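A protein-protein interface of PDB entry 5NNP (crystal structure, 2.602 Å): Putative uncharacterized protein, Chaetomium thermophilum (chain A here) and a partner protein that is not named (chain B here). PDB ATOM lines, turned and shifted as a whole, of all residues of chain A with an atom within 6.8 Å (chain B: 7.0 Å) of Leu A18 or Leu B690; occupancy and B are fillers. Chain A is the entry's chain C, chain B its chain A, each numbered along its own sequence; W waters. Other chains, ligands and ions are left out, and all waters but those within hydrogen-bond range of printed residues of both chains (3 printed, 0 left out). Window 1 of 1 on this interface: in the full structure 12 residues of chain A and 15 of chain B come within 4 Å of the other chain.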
ATOM      1  N   LEU A  13      32.364   1.905 -22.715  1.00  0.00           N
ATOM      2  CA  LEU A  13      31.874   3.223 -22.361  1.00  0.00           C
ATOM      3  C   LEU A  13      30.411   3.347 -22.765  1.00  0.00           C
ATOM      4  O   LEU A  13      29.580   3.764 -21.965  1.00  0.00           O
ATOM      5  CB  LEU A  13      32.703   4.318 -23.026  1.00  0.00           C
ATOM      6  CG  LEU A  13      32.210   5.741 -22.735  1.00  0.00           C
ATOM      7  CD1 LEU A  13      32.568   6.180 -21.321  1.00  0.00           C
ATOM      8  CD2 LEU A  13      32.759   6.721 -23.767  1.00  0.00           C
ATOM      9  N   LEU A  14      30.098   2.975 -24.001  1.00  0.00           N
ATOM     10  CA  LEU A  14      28.711   3.014 -24.468  1.00  0.00           C
ATOM     11  C   LEU A  14      27.820   2.066 -23.675  1.00  0.00           C
ATOM     12  O   LEU A  14      26.655   2.376 -23.416  1.00  0.00           O
ATOM     13  CB  LEU A  14      28.625   2.679 -25.956  1.00  0.00           C
ATOM     14  CG  LEU A  14      28.823   3.851 -26.917  1.00  0.00           C
ATOM     15  CD1 LEU A  14      30.202   4.449 -26.773  1.00  0.00           C
ATOM     16  CD2 LEU A  14      28.619   3.382 -28.328  1.00  0.00           C
ATOM     17  N   VAL A  15      28.367   0.918 -23.287  1.00  0.00           N
ATOM     18  CA  VAL A  15      27.598  -0.054 -22.517  1.00  0.00           C
ATOM     19  C   VAL A  15      27.178   0.569 -21.193  1.00  0.00           C
ATOM     20  O   VAL A  15      26.006   0.542 -20.829  1.00  0.00           O
ATOM     21  CB  VAL A  15      28.389  -1.364 -22.257  1.00  0.00           C
ATOM     22  CG1 VAL A  15      27.730  -2.170 -21.156  1.00  0.00           C
ATOM     23  CG2 VAL A  15      28.473  -2.198 -23.524  1.00  0.00           C
ATOM     24  N   GLU A  16      28.139   1.165 -20.499  1.00  0.00           N
ATOM     25  CA  GLU A  16      27.886   1.745 -19.189  1.00  0.00           C
ATOM     26  C   GLU A  16      27.034   3.021 -19.232  1.00  0.00           C
ATOM     27  O   GLU A  16      26.204   3.246 -18.349  1.00  0.00           O
ATOM     28  CB  GLU A  16      29.218   2.027 -18.487  1.00  0.00           C
ATOM     29  CG  GLU A  16      29.118   2.974 -17.305  1.00  0.00           C
ATOM     30  CD  GLU A  16      28.528   2.328 -16.059  1.00  0.00           C
ATOM     31  OE1 GLU A  16      28.474   1.077 -15.989  1.00  0.00           O
ATOM     32  OE2 GLU A  16      28.121   3.081 -15.146  1.00  0.00           O
ATOM     33  N   GLU A  17      27.231   3.859 -20.244  1.00  0.00           N
ATOM     34  CA  GLU A  17      26.628   5.195 -20.211  1.00  0.00           C
ATOM     35  C   GLU A  17      25.350   5.291 -21.042  1.00  0.00           C
ATOM     36  O   GLU A  17      24.604   6.254 -20.917  1.00  0.00           O
ATOM     37  CB  GLU A  17      27.635   6.259 -20.683  1.00  0.00           C
ATOM     38  CG  GLU A  17      28.874   6.425 -19.798  1.00  0.00           C
ATOM     39  CD  GLU A  17      28.553   6.971 -18.411  1.00  0.00           C
ATOM     40  OE1 GLU A  17      29.196   6.530 -17.432  1.00  0.00           O
ATOM     41  OE2 GLU A  17      27.668   7.847 -18.294  1.00  0.00           O
ATOM     42  N   LEU A  18      25.108   4.299 -21.898  1.00  0.00           N
ATOM     43  CA  LEU A  18      23.869   4.246 -22.683  1.00  0.00           C
ATOM     44  C   LEU A  18      23.035   3.035 -22.288  1.00  0.00           C
ATOM     45  O   LEU A  18      21.894   2.892 -22.705  1.00  0.00           O
ATOM     46  CB  LEU A  18      24.168   4.210 -24.181  1.00  0.00           C
ATOM     47  CG  LEU A  18      24.796   5.501 -24.708  1.00  0.00           C
ATOM     48  CD1 LEU A  18      25.210   5.392 -26.168  1.00  0.00           C
ATOM     49  CD2 LEU A  18      23.842   6.680 -24.487  1.00  0.00           C
ATOM     50  N   GLU A  19      23.623   2.170 -21.472  1.00  0.00           N
ATOM     51  CA  GLU A  19      22.939   0.996 -20.952  1.00  0.00           C
ATOM     52  C   GLU A  19      22.541   0.083 -22.100  1.00  0.00           C
ATOM     53  O   GLU A  19      21.430  -0.425 -22.152  1.00  0.00           O
ATOM     54  CB  GLU A  19      21.722   1.401 -20.098  1.00  0.00           C
ATOM     55  CG  GLU A  19      22.102   2.280 -18.890  1.00  0.00           C
ATOM     56  CD  GLU A  19      21.101   2.252 -17.743  1.00  0.00           C
ATOM     57  OE1 GLU A  19      19.875   2.243 -18.007  1.00  0.00           O
ATOM     58  OE2 GLU A  19      21.550   2.250 -16.574  1.00  0.00           O
ATOM     59  N   LEU A  20      23.479  -0.118 -23.018  1.00  0.00           N
ATOM     60  CA  LEU A  20      23.275  -0.986 -24.165  1.00  0.00           C
ATOM     61  C   LEU A  20      23.975  -2.329 -23.997  1.00  0.00           C
ATOM     62  O   LEU A  20      24.951  -2.444 -23.269  1.00  0.00           O
ATOM     63  CB  LEU A  20      23.780  -0.304 -25.431  1.00  0.00           C
ATOM     64  CG  LEU A  20      23.109   1.022 -25.761  1.00  0.00           C
ATOM     65  CD1 LEU A  20      23.554   1.494 -27.122  1.00  0.00           C
ATOM     66  CD2 LEU A  20      21.614   0.870 -25.724  1.00  0.00           C
ATOM     67  N   SER A  21      23.471  -3.345 -24.683  1.00  0.00           N
ATOM     68  CA  SER A  21      24.159  -4.624 -24.760  1.00  0.00           C
ATOM     69  C   SER A  21      25.466  -4.424 -25.493  1.00  0.00           C
ATOM     70  O   SER A  21      25.578  -3.520 -26.318  1.00  0.00           O
ATOM     71  CB  SER A  21      23.306  -5.663 -25.487  1.00  0.00           C
ATOM     72  OG  SER A  21      23.131  -5.304 -26.851  1.00  0.00           O
ATOM     73  N   ALA A  25      25.956  -1.854 -28.599  1.00  0.00           N
ATOM     74  CA  ALA A  25      26.887  -0.758 -28.420  1.00  0.00           C
ATOM     75  C   ALA A  25      27.913  -0.806 -29.536  1.00  0.00           C
ATOM     76  O   ALA A  25      28.279   0.219 -30.120  1.00  0.00           O
ATOM     77  CB  ALA A  25      27.548  -0.838 -27.068  1.00  0.00           C
ATOM     78  N   LEU A  28      26.333   0.129 -32.871  1.00  0.00           N
ATOM     79  CA  LEU A  28      26.139   1.576 -32.959  1.00  0.00           C
ATOM     80  C   LEU A  28      27.459   2.233 -33.308  1.00  0.00           C
ATOM     81  O   LEU A  28      27.520   3.098 -34.179  1.00  0.00           O
ATOM     82  CB  LEU A  28      25.576   2.157 -31.651  1.00  0.00           C
ATOM     83  CG  LEU A  28      25.448   3.694 -31.537  1.00  0.00           C
ATOM     84  CD1 LEU A  28      24.550   4.251 -32.614  1.00  0.00           C
ATOM     85  CD2 LEU A  28      24.947   4.158 -30.158  1.00  0.00           C
ATOM     86  N   ALA A  39      29.012   8.685 -32.355  1.00  0.00           N
ATOM     87  CA  ALA A  39      27.924   7.745 -32.071  1.00  0.00           C
ATOM     88  C   ALA A  39      27.051   8.201 -30.889  1.00  0.00           C
ATOM     89  O   ALA A  39      25.825   8.163 -30.971  1.00  0.00           O
ATOM     90  CB  ALA A  39      28.484   6.351 -31.813  1.00  0.00           C
ATOM     91  N   MET A  40      27.678   8.635 -29.798  1.00  0.00           N
ATOM     92  CA  MET A  40      26.935   9.104 -28.627  1.00  0.00           C
ATOM     93  C   MET A  40      26.089  10.347 -28.928  1.00  0.00           C
ATOM     94  O   MET A  40      24.965  10.481 -28.440  1.00  0.00           O
ATOM     95  CB  MET A  40      27.890   9.411 -27.467  1.00  0.00           C
ATOM     96  CG  MET A  40      28.501   8.187 -26.785  1.00  0.00           C
ATOM     97  SD  MET A  40      29.452   8.633 -25.320  1.00  0.00           S
ATOM     98  CE  MET A  40      30.958   9.272 -26.035  1.00  0.00           C
ATOM     99  N   LYS A  41      26.630  11.263 -29.724  1.00  0.00           N
ATOM    100  CA  LYS A  41      25.889  12.463 -30.087  1.00  0.00           C
ATOM    101  C   LYS A  41      24.677  12.121 -30.963  1.00  0.00           C
ATOM    102  O   LYS A  41      23.609  12.712 -30.822  1.00  0.00           O
ATOM    103  CB  LYS A  41      26.799  13.457 -30.808  1.00  0.00           C
ATOM    104  CG  LYS A  41      27.835  14.135 -29.928  1.00  0.00           C
ATOM    105  CD  LYS A  41      28.569  15.201 -30.726  1.00  0.00           C
ATOM    106  CE  LYS A  41      29.415  16.100 -29.856  1.00  0.00           C
ATOM    107  NZ  LYS A  41      29.838  17.292 -30.633  1.00  0.00           N
ATOM    108  N   TYR A  43      23.013   9.182 -31.114  1.00  0.00           N
ATOM    109  CA  TYR A  43      22.076   8.407 -30.316  1.00  0.00           C
ATOM    110  C   TYR A  43      21.140   9.229 -29.432  1.00  0.00           C
ATOM    111  O   TYR A  43      20.009   8.821 -29.215  1.00  0.00           O
ATOM    112  CB  TYR A  43      22.847   7.421 -29.437  1.00  0.00           C
ATOM    113  CG  TYR A  43      21.950   6.435 -28.733  1.00  0.00           C
ATOM    114  CD1 TYR A  43      21.468   6.688 -27.455  1.00  0.00           C
ATOM    115  CD2 TYR A  43      21.567   5.262 -29.352  1.00  0.00           C
ATOM    116  CE1 TYR A  43      20.635   5.791 -26.813  1.00  0.00           C
ATOM    117  CE2 TYR A  43      20.748   4.369 -28.724  1.00  0.00           C
ATOM    118  CZ  TYR A  43      20.277   4.633 -27.458  1.00  0.00           C
ATOM    119  OH  TYR A  43      19.457   3.720 -26.841  1.00  0.00           O
ATOM    120  N   ILE A  44      21.601  10.364 -28.904  1.00  0.00           N
ATOM    121  CA  ILE A  44      20.759  11.183 -28.018  1.00  0.00           C
ATOM    122  C   ILE A  44      19.947  12.259 -28.754  1.00  0.00           C
ATOM    123  O   ILE A  44      19.269  13.063 -28.120  1.00  0.00           O
ATOM    124  CB  ILE A  44      21.584  11.890 -26.915  1.00  0.00           C
ATOM    125  CG1 ILE A  44      22.699  12.750 -27.527  1.00  0.00           C
ATOM    126  CG2 ILE A  44      22.135  10.885 -25.916  1.00  0.00           C
ATOM    127  CD1 ILE A  44      23.394  13.650 -26.531  1.00  0.00           C
ATOM    128  N   TYR B 683      17.086   8.832 -14.550  1.00  0.00           N
ATOM    129  CA  TYR B 683      18.493   8.741 -14.953  1.00  0.00           C
ATOM    130  C   TYR B 683      19.473   9.624 -14.170  1.00  0.00           C
ATOM    131  O   TYR B 683      20.620   9.218 -13.956  1.00  0.00           O
ATOM    132  CB  TYR B 683      18.631   9.050 -16.442  1.00  0.00           C
ATOM    133  CG  TYR B 683      18.098   7.948 -17.324  1.00  0.00           C
ATOM    134  CD1 TYR B 683      18.434   6.626 -17.089  1.00  0.00           C
ATOM    135  CD2 TYR B 683      17.249   8.230 -18.382  1.00  0.00           C
ATOM    136  CE1 TYR B 683      17.951   5.614 -17.893  1.00  0.00           C
ATOM    137  CE2 TYR B 683      16.763   7.228 -19.188  1.00  0.00           C
ATOM    138  CZ  TYR B 683      17.116   5.920 -18.938  1.00  0.00           C
ATOM    139  OH  TYR B 683      16.633   4.918 -19.740  1.00  0.00           O
ATOM    140  N   LYS B 687      22.642   8.177 -11.900  1.00  0.00           N
ATOM    141  CA  LYS B 687      23.960   8.727 -12.238  1.00  0.00           C
ATOM    142  C   LYS B 687      24.340   8.512 -13.708  1.00  0.00           C
ATOM    143  O   LYS B 687      25.520   8.564 -14.071  1.00  0.00           O
ATOM    144  CB  LYS B 687      25.047   8.127 -11.341  1.00  0.00           C
ATOM    145  CG  LYS B 687      24.788   8.258  -9.853  1.00  0.00           C
ATOM    146  CD  LYS B 687      24.590   9.702  -9.455  1.00  0.00           C
ATOM    147  CE  LYS B 687      24.502   9.833  -7.942  1.00  0.00           C
ATOM    148  NZ  LYS B 687      25.688   9.222  -7.277  1.00  0.00           N
ATOM    149  N   LYS B 688      23.340   8.274 -14.546  1.00  0.00           N
ATOM    150  CA  LYS B 688      23.560   8.084 -15.972  1.00  0.00           C
ATOM    151  C   LYS B 688      23.186   9.358 -16.714  1.00  0.00           C
ATOM    152  O   LYS B 688      22.117   9.460 -17.303  1.00  0.00           O
ATOM    153  CB  LYS B 688      22.757   6.890 -16.492  1.00  0.00           C
ATOM    154  CG  LYS B 688      23.167   5.549 -15.884  1.00  0.00           C
ATOM    155  CD  LYS B 688      24.637   5.211 -16.188  1.00  0.00           C
ATOM    156  CE  LYS B 688      25.124   3.963 -15.437  1.00  0.00           C
ATOM    157  NZ  LYS B 688      24.372   2.718 -15.782  1.00  0.00           N
ATOM    158  N   TYR B 689      24.098  10.321 -16.690  1.00  0.00           N
ATOM    159  CA  TYR B 689      23.826  11.673 -17.160  1.00  0.00           C
ATOM    160  C   TYR B 689      23.669  11.791 -18.678  1.00  0.00           C
ATOM    161  O   TYR B 689      23.119  12.778 -19.164  1.00  0.00           O
ATOM    162  CB  TYR B 689      24.935  12.608 -16.676  1.00  0.00           C
ATOM    163  CG  TYR B 689      25.149  12.552 -15.178  1.00  0.00           C
ATOM    164  CD1 TYR B 689      24.108  12.851 -14.299  1.00  0.00           C
ATOM    165  CD2 TYR B 689      26.382  12.201 -14.641  1.00  0.00           C
ATOM    166  CE1 TYR B 689      24.284  12.799 -12.933  1.00  0.00           C
ATOM    167  CE2 TYR B 689      26.568  12.150 -13.278  1.00  0.00           C
ATOM    168  CZ  TYR B 689      25.513  12.452 -12.429  1.00  0.00           C
ATOM    169  OH  TYR B 689      25.682  12.405 -11.066  1.00  0.00           O
ATOM    170  N   LEU B 690      24.146  10.802 -19.428  1.00  0.00           N
ATOM    171  CA  LEU B 690      24.004  10.839 -20.879  1.00  0.00           C
ATOM    172  C   LEU B 690      22.563  10.508 -21.307  1.00  0.00           C
ATOM    173  O   LEU B 690      22.008  11.136 -22.211  1.00  0.00           O
ATOM    174  CB  LEU B 690      24.986   9.877 -21.540  1.00  0.00           C
ATOM    175  CG  LEU B 690      25.116  10.081 -23.048  1.00  0.00           C
ATOM    176  CD1 LEU B 690      25.421  11.536 -23.357  1.00  0.00           C
ATOM    177  CD2 LEU B 690      26.176   9.172 -23.651  1.00  0.00           C
ATOM    178  N   LEU B 691      21.960   9.522 -20.650  1.00  0.00           N
ATOM    179  CA  LEU B 691      20.575   9.170 -20.920  1.00  0.00           C
ATOM    180  C   LEU B 691      19.643  10.265 -20.418  1.00  0.00           C
ATOM    181  O   LEU B 691      18.638  10.581 -21.048  1.00  0.00           O
ATOM    182  CB  LEU B 691      20.223   7.827 -20.274  1.00  0.00           C
ATOM    183  CG  LEU B 691      21.040   6.642 -20.795  1.00  0.00           C
ATOM    184  CD1 LEU B 691      20.533   5.326 -20.220  1.00  0.00           C
ATOM    185  CD2 LEU B 691      21.004   6.625 -22.310  1.00  0.00           C
ATOM    186  N   ALA B 692      19.989  10.838 -19.271  1.00  0.00           N
ATOM    187  CA  ALA B 692      19.268  11.986 -18.737  1.00  0.00           C
ATOM    188  C   ALA B 692      19.153  13.091 -19.786  1.00  0.00           C
ATOM    189  O   ALA B 692      18.068  13.617 -20.025  1.00  0.00           O
ATOM    190  CB  ALA B 692      19.962  12.511 -17.474  1.00  0.00           C
ATOM    191  N   LEU B 693      20.278  13.428 -20.414  1.00  0.00           N
ATOM    192  CA  LEU B 693      20.305  14.452 -21.447  1.00  0.00           C
ATOM    193  C   LEU B 693      19.431  14.070 -22.634  1.00  0.00           C
ATOM    194  O   LEU B 693      18.781  14.918 -23.250  1.00  0.00           O
ATOM    195  CB  LEU B 693      21.733  14.691 -21.915  1.00  0.00           C
ATOM    196  CG  LEU B 693      21.892  15.766 -22.982  1.00  0.00           C
ATOM    197  CD1 LEU B 693      21.297  17.077 -22.497  1.00  0.00           C
ATOM    198  CD2 LEU B 693      23.360  15.936 -23.325  1.00  0.00           C
ATOM    199  N   ARG B 694      19.418  12.784 -22.954  1.00  0.00           N
ATOM    200  CA  ARG B 694      18.669  12.308 -24.101  1.00  0.00           C
ATOM    201  C   ARG B 694      17.185  12.549 -23.900  1.00  0.00           C
ATOM    202  O   ARG B 694      16.506  13.051 -24.795  1.00  0.00           O
ATOM    203  CB  ARG B 694      18.948  10.839 -24.327  1.00  0.00           C
ATOM    204  CG  ARG B 694      18.198  10.208 -25.467  1.00  0.00           C
ATOM    205  CD  ARG B 694      18.709   8.797 -25.602  1.00  0.00           C
ATOM    206  NE  ARG B 694      18.067   8.034 -26.658  1.00  0.00           N
ATOM    207  CZ  ARG B 694      17.198   7.054 -26.450  1.00  0.00           C
ATOM    208  NH1 ARG B 694      16.841   6.716 -25.216  1.00  0.00           N
ATOM    209  NH2 ARG B 694      16.684   6.416 -27.487  1.00  0.00           N
ATOM    210  N   CYS B 695      16.699  12.183 -22.714  1.00  0.00           N
ATOM    211  CA  CYS B 695      15.347  12.507 -22.277  1.00  0.00           C
ATOM    212  C   CYS B 695      15.070  13.999 -22.328  1.00  0.00           C
ATOM    213  O   CYS B 695      14.048  14.428 -22.859  1.00  0.00           O
ATOM    214  CB  CYS B 695      15.114  12.008 -20.857  1.00  0.00           C
ATOM    215  SG  CYS B 695      14.948  10.239 -20.735  1.00  0.00           S
ATOM    216  N   LEU B 716      20.245  19.945 -14.293  1.00  0.00           N
ATOM    217  CA  LEU B 716      21.271  19.108 -14.902  1.00  0.00           C
ATOM    218  C   LEU B 716      22.604  19.832 -14.957  1.00  0.00           C
ATOM    219  O   LEU B 716      23.646  19.275 -14.615  1.00  0.00           O
ATOM    220  CB  LEU B 716      20.846  18.692 -16.311  1.00  0.00           C
ATOM    221  CG  LEU B 716      21.609  17.580 -17.028  1.00  0.00           C
ATOM    222  CD1 LEU B 716      21.362  16.222 -16.374  1.00  0.00           C
ATOM    223  CD2 LEU B 716      21.192  17.552 -18.489  1.00  0.00           C
ATOM    224  N   LEU B 731      32.860  11.314 -22.626  1.00  0.00           N
ATOM    225  CA  LEU B 731      31.535  11.590 -22.078  1.00  0.00           C
ATOM    226  C   LEU B 731      31.395  13.072 -21.725  1.00  0.00           C
ATOM    227  O   LEU B 731      30.394  13.718 -22.045  1.00  0.00           O
ATOM    228  CB  LEU B 731      31.291  10.720 -20.843  1.00  0.00           C
ATOM    229  CG  LEU B 731      29.997  10.896 -20.055  1.00  0.00           C
ATOM    230  CD1 LEU B 731      28.812  10.484 -20.913  1.00  0.00           C
ATOM    231  CD2 LEU B 731      30.061  10.079 -18.778  1.00  0.00           C
ATOM    232  N   VAL B 734      30.856  15.109 -25.010  1.00  0.00           N
ATOM    233  CA  VAL B 734      29.555  14.978 -25.640  1.00  0.00           C
ATOM    234  C   VAL B 734      28.492  15.681 -24.815  1.00  0.00           C
ATOM    235  O   VAL B 734      27.586  16.319 -25.354  1.00  0.00           O
ATOM    236  CB  VAL B 734      29.156  13.500 -25.820  1.00  0.00           C
ATOM    237  CG1 VAL B 734      27.701  13.388 -26.263  1.00  0.00           C
ATOM    238  CG2 VAL B 734      30.082  12.807 -26.800  1.00  0.00           C
ATOM    239  N   ILE B 735      28.611  15.546 -23.499  1.00  0.00           N
ATOM    240  CA  ILE B 735      27.679  16.163 -22.559  1.00  0.00           C
ATOM    241  C   ILE B 735      27.636  17.683 -22.735  1.00  0.00           C
ATOM    242  O   ILE B 735      26.584  18.254 -23.032  1.00  0.00           O
ATOM    243  CB  ILE B 735      28.061  15.831 -21.098  1.00  0.00           C
ATOM    244  CG1 ILE B 735      27.744  14.368 -20.775  1.00  0.00           C
ATOM    245  CG2 ILE B 735      27.341  16.757 -20.134  1.00  0.00           C
ATOM    246  CD1 ILE B 735      26.309  14.079 -20.659  1.00  0.00           C
ATOM    247  N   GLU B 738      26.368  18.913 -26.410  1.00  0.00           N
ATOM    248  CA  GLU B 738      24.957  18.781 -26.753  1.00  0.00           C
ATOM    249  C   GLU B 738      24.050  19.416 -25.712  1.00  0.00           C
ATOM    250  O   GLU B 738      22.833  19.450 -25.878  1.00  0.00           O
ATOM    251  CB  GLU B 738      24.592  17.307 -26.924  1.00  0.00           C
ATOM    252  CG  GLU B 738      25.275  16.650 -28.104  1.00  0.00           C
ATOM    253  CD  GLU B 738      24.758  17.152 -29.440  1.00  0.00           C
ATOM    254  OE1 GLU B 738      25.560  17.212 -30.399  1.00  0.00           O
ATOM    255  OE2 GLU B 738      23.554  17.480 -29.532  1.00  0.00           O
HETATM  256  O   HOH W   1      16.655  12.951 -27.468  1.00  0.00           O
HETATM  257  O   HOH W   2      18.270   2.572 -19.771  1.00  0.00           O
HETATM  258  O   HOH W   3      24.688   7.998 -18.786  1.00  0.00           O
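The side-chain amino group (NZ) of Lys B688 is in salt-bridge range of the side-chain carboxylate (OE2) of Glu A16. The side-chain carboxylate (OE2) of Glu A19 lies within salt-bridge range of the side-chain amino group (NZ) of Lys B688 (3.0 Å). The guanidinium group (NE) of Arg B694 sits at hydrogen-bond distance from the backbone carbonyl oxygen (O) of Tyr A43 (3.3 Å).
The backbone carbonyl oxygen (O) of Tyr B683 sits at hydrogen-bond distance from the backbone NH (N) of Lys B688 (2.9 Å). The side-chain sulfur (SG) of Cys B695 lies within hydrogen-bond range of the backbone carbonyl oxygen (O) of Leu B691.
Leu B691 touches Glu A17 (CG to O, 3.6 Å). CD2 of Leu B690 touches CD2 of Leu A18, 3.5 Å away. CD2 of Leu A18 touches CD2 of Leu B691, at 3.6 Å. Glu A19 touches Tyr B683 (OE1 to CE1, 3.9 Å). Met A40 touches Leu B690 (SD to CD2, 3.7 Å). Met A40 touches Val B734. Val B734 touches Lys A41 (CG1 to CG, 3.7 Å). Lys A41 touches Glu B738. Leu B693 touches Ile A44 (CD2 to CD1, 3.9 Å). Ile A44 touches Glu B738 (CD1 to CB, 3.9 Å).
Of the printed residues of chain B, Glu A19 touches Tyr B683 (3.9 Å), Lys B688 (3.0 Å) and Leu B691 (3.7 Å). Leu A20 touches none of the printed residues of chain B. Printed residues of chain B within 4 Å of Met A40: Leu B690 and Val B734. Leu B690 touches just these residues of chain A: Glu A17, Leu A18, Met A40 and Ile A44. Leu B716 touches none of the printed residues of chain A. The nearest residue of chain B that does not touch Leu A18 is Arg B694 (5.7 Å). The nearest printed residue of chain A that does not touch Leu B691 is Tyr A43 (4.6 Å).
Of the 16 printed residues of chain A, 8 touch a printed residue of chain B. Hydrophobic or aromatic side chains of chain A within 4 Å of the printed part of chain B: Leu A18, Met A40, Tyr A43 and Ile A44. Of the 15 printed residues of chain B, 9 touch a printed residue of chain A.
Water W2 lies within hydrogen-bond range of the side-chain carboxylate of Glu A19 and the side-chain hydroxyl of Tyr B683. Water W1 bridges the backbone carbonyl oxygen (O) of Arg B694 (2.7 Å) and the backbone carbonyl oxygen (O) of Ile A44 (2.7 Å). Water W3 lies within hydrogen-bond range of O of Glu A17 (2.8 Å), N of Leu B690 (2.9 Å), N of Tyr B689 (3.2 Å) and O of Lys B688 (3.3 Å).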
